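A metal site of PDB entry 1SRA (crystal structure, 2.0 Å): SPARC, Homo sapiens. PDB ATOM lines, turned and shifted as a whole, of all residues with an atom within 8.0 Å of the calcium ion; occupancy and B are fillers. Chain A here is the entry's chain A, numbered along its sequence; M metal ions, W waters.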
ATOM      1  N   LEU A 103      18.277  -6.973 -18.438  1.00  0.00           N
ATOM      2  CA  LEU A 103      19.500  -7.506 -19.016  1.00  0.00           C
ATOM      3  C   LEU A 103      19.624  -9.003 -18.812  1.00  0.00           C
ATOM      4  O   LEU A 103      20.586  -9.617 -19.267  1.00  0.00           O
ATOM      5  CB  LEU A 103      20.746  -6.775 -18.497  1.00  0.00           C
ATOM      6  CG  LEU A 103      20.761  -5.277 -18.832  1.00  0.00           C
ATOM      7  CD1 LEU A 103      22.069  -4.626 -18.396  1.00  0.00           C
ATOM      8  CD2 LEU A 103      20.537  -5.111 -20.335  1.00  0.00           C
ATOM      9  N   ARG A 104      18.676  -9.588 -18.086  1.00  0.00           N
ATOM     10  CA  ARG A 104      18.645 -11.026 -17.853  1.00  0.00           C
ATOM     11  C   ARG A 104      17.600 -11.710 -18.783  1.00  0.00           C
ATOM     12  O   ARG A 104      17.278 -12.891 -18.624  1.00  0.00           O
ATOM     13  CB  ARG A 104      18.329 -11.341 -16.393  1.00  0.00           C
ATOM     14  CG  ARG A 104      19.420 -10.917 -15.431  1.00  0.00           C
ATOM     15  CD  ARG A 104      19.240 -11.507 -14.046  1.00  0.00           C
ATOM     16  NE  ARG A 104      18.006 -11.062 -13.382  1.00  0.00           N
ATOM     17  CZ  ARG A 104      17.906  -9.974 -12.619  1.00  0.00           C
ATOM     18  NH1 ARG A 104      18.967  -9.202 -12.410  1.00  0.00           N
ATOM     19  NH2 ARG A 104      16.771  -9.692 -11.995  1.00  0.00           N
ATOM     20  N   ALA A 105      17.090 -10.967 -19.753  1.00  0.00           N
ATOM     21  CA  ALA A 105      16.113 -11.508 -20.702  1.00  0.00           C
ATOM     22  C   ALA A 105      16.804 -12.298 -21.846  1.00  0.00           C
ATOM     23  O   ALA A 105      17.928 -11.959 -22.267  1.00  0.00           O
ATOM     24  CB  ALA A 105      15.243 -10.371 -21.251  1.00  0.00           C
ATOM     25  N   PRO A 106      16.172 -13.382 -22.331  1.00  0.00           N
ATOM     26  CA  PRO A 106      16.668 -14.253 -23.393  1.00  0.00           C
ATOM     27  C   PRO A 106      17.224 -13.587 -24.625  1.00  0.00           C
ATOM     28  O   PRO A 106      18.157 -14.081 -25.211  1.00  0.00           O
ATOM     29  CB  PRO A 106      15.478 -15.147 -23.741  1.00  0.00           C
ATOM     30  CG  PRO A 106      14.347 -14.609 -22.954  1.00  0.00           C
ATOM     31  CD  PRO A 106      14.948 -13.976 -21.763  1.00  0.00           C
ATOM     32  N   LEU A 107      16.734 -12.414 -24.969  1.00  0.00           N
ATOM     33  CA  LEU A 107      17.259 -11.819 -26.174  1.00  0.00           C
ATOM     34  C   LEU A 107      18.544 -10.995 -26.003  1.00  0.00           C
ATOM     35  O   LEU A 107      19.054 -10.393 -26.956  1.00  0.00           O
ATOM     36  CB  LEU A 107      16.157 -11.076 -26.933  1.00  0.00           C
ATOM     37  CG  LEU A 107      14.880 -11.942 -27.087  1.00  0.00           C
ATOM     38  CD1 LEU A 107      14.126 -11.548 -28.335  1.00  0.00           C
ATOM     39  CD2 LEU A 107      15.216 -13.423 -27.190  1.00  0.00           C
ATOM     40  N   ILE A 108      19.100 -11.034 -24.794  1.00  0.00           N
ATOM     41  CA  ILE A 108      20.342 -10.300 -24.521  1.00  0.00           C
ATOM     42  C   ILE A 108      21.472 -11.266 -24.840  1.00  0.00           C
ATOM     43  O   ILE A 108      21.452 -12.416 -24.430  1.00  0.00           O
ATOM     44  CB  ILE A 108      20.451  -9.920 -23.000  1.00  0.00           C
ATOM     45  CG1 ILE A 108      19.306  -9.015 -22.576  1.00  0.00           C
ATOM     46  CG2 ILE A 108      21.763  -9.272 -22.708  1.00  0.00           C
ATOM     47  CD1 ILE A 108      19.259  -7.718 -23.291  1.00  0.00           C
ATOM     48  N   PRO A 109      22.504 -10.797 -25.564  1.00  0.00           N
ATOM     49  CA  PRO A 109      23.553 -11.770 -25.824  1.00  0.00           C
ATOM     50  C   PRO A 109      24.208 -12.253 -24.532  1.00  0.00           C
ATOM     51  O   PRO A 109      24.446 -11.453 -23.628  1.00  0.00           O
ATOM     52  CB  PRO A 109      24.543 -10.992 -26.687  1.00  0.00           C
ATOM     53  CG  PRO A 109      24.025  -9.617 -26.779  1.00  0.00           C
ATOM     54  CD  PRO A 109      22.646  -9.551 -26.318  1.00  0.00           C
ATOM     55  N   MET A 110      24.465 -13.548 -24.430  1.00  0.00           N
ATOM     56  CA  MET A 110      25.092 -14.149 -23.261  1.00  0.00           C
ATOM     57  C   MET A 110      24.386 -13.774 -21.975  1.00  0.00           C
ATOM     58  O   MET A 110      25.022 -13.607 -20.938  1.00  0.00           O
ATOM     59  CB  MET A 110      26.540 -13.707 -23.178  1.00  0.00           C
ATOM     60  CG  MET A 110      27.247 -13.727 -24.517  1.00  0.00           C
ATOM     61  SD  MET A 110      29.015 -13.549 -24.356  1.00  0.00           S
ATOM     62  CE  MET A 110      29.382 -15.079 -23.695  1.00  0.00           C
ATOM     63  N   GLU A 111      23.069 -13.682 -22.036  1.00  0.00           N
ATOM     64  CA  GLU A 111      22.308 -13.286 -20.870  1.00  0.00           C
ATOM     65  C   GLU A 111      22.488 -14.212 -19.665  1.00  0.00           C
ATOM     66  O   GLU A 111      22.126 -13.828 -18.566  1.00  0.00           O
ATOM     67  CB  GLU A 111      20.819 -13.092 -21.222  1.00  0.00           C
ATOM     68  CG  GLU A 111      19.895 -14.290 -20.986  1.00  0.00           C
ATOM     69  CD  GLU A 111      20.070 -15.469 -21.983  1.00  0.00           C
ATOM     70  OE1 GLU A 111      20.747 -15.316 -23.025  1.00  0.00           O
ATOM     71  OE2 GLU A 111      19.504 -16.547 -21.720  1.00  0.00           O
ATOM     72  N   HIS A 112      23.015 -15.424 -19.858  1.00  0.00           N
ATOM     73  CA  HIS A 112      23.228 -16.331 -18.717  1.00  0.00           C
ATOM     74  C   HIS A 112      24.481 -15.907 -17.913  1.00  0.00           C
ATOM     75  O   HIS A 112      24.764 -16.443 -16.864  1.00  0.00           O
ATOM     76  CB  HIS A 112      23.342 -17.807 -19.163  1.00  0.00           C
ATOM     77  CG  HIS A 112      24.553 -18.082 -19.992  1.00  0.00           C
ATOM     78  ND1 HIS A 112      24.775 -17.460 -21.207  1.00  0.00           N
ATOM     79  CD2 HIS A 112      25.641 -18.855 -19.759  1.00  0.00           C
ATOM     80  CE1 HIS A 112      25.943 -17.843 -21.690  1.00  0.00           C
ATOM     81  NE2 HIS A 112      26.493 -18.678 -20.830  1.00  0.00           N
HETATM   82 CA    CA M   1      20.372 -14.593 -25.418  1.00  0.00          CA
HETATM   83  O   HOH W   1      19.461 -17.404 -26.842  1.00  0.00           O
HETATM   84  O   HOH W   2      20.499 -12.985 -27.715  1.00  0.00           O
HETATM   85  O   HOH W   3      23.090 -15.682 -25.953  1.00  0.00           O
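Three residues have an atom within 4 Å of the calcium ion: Pro 106, Ile 108 and Glu 111. The nearest printed residue that does not touch the calcium ion is Leu 107 (4.1 Å).
The calcium ion is bound by O of Pro 106 (2.3 Å), OE1 of Glu 111 (2.5 Å), O of Ile 108 (2.6 Å) and water W2 (2.8 Å). Slightly farther from the calcium ion lies water W3 (3.0 Å).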
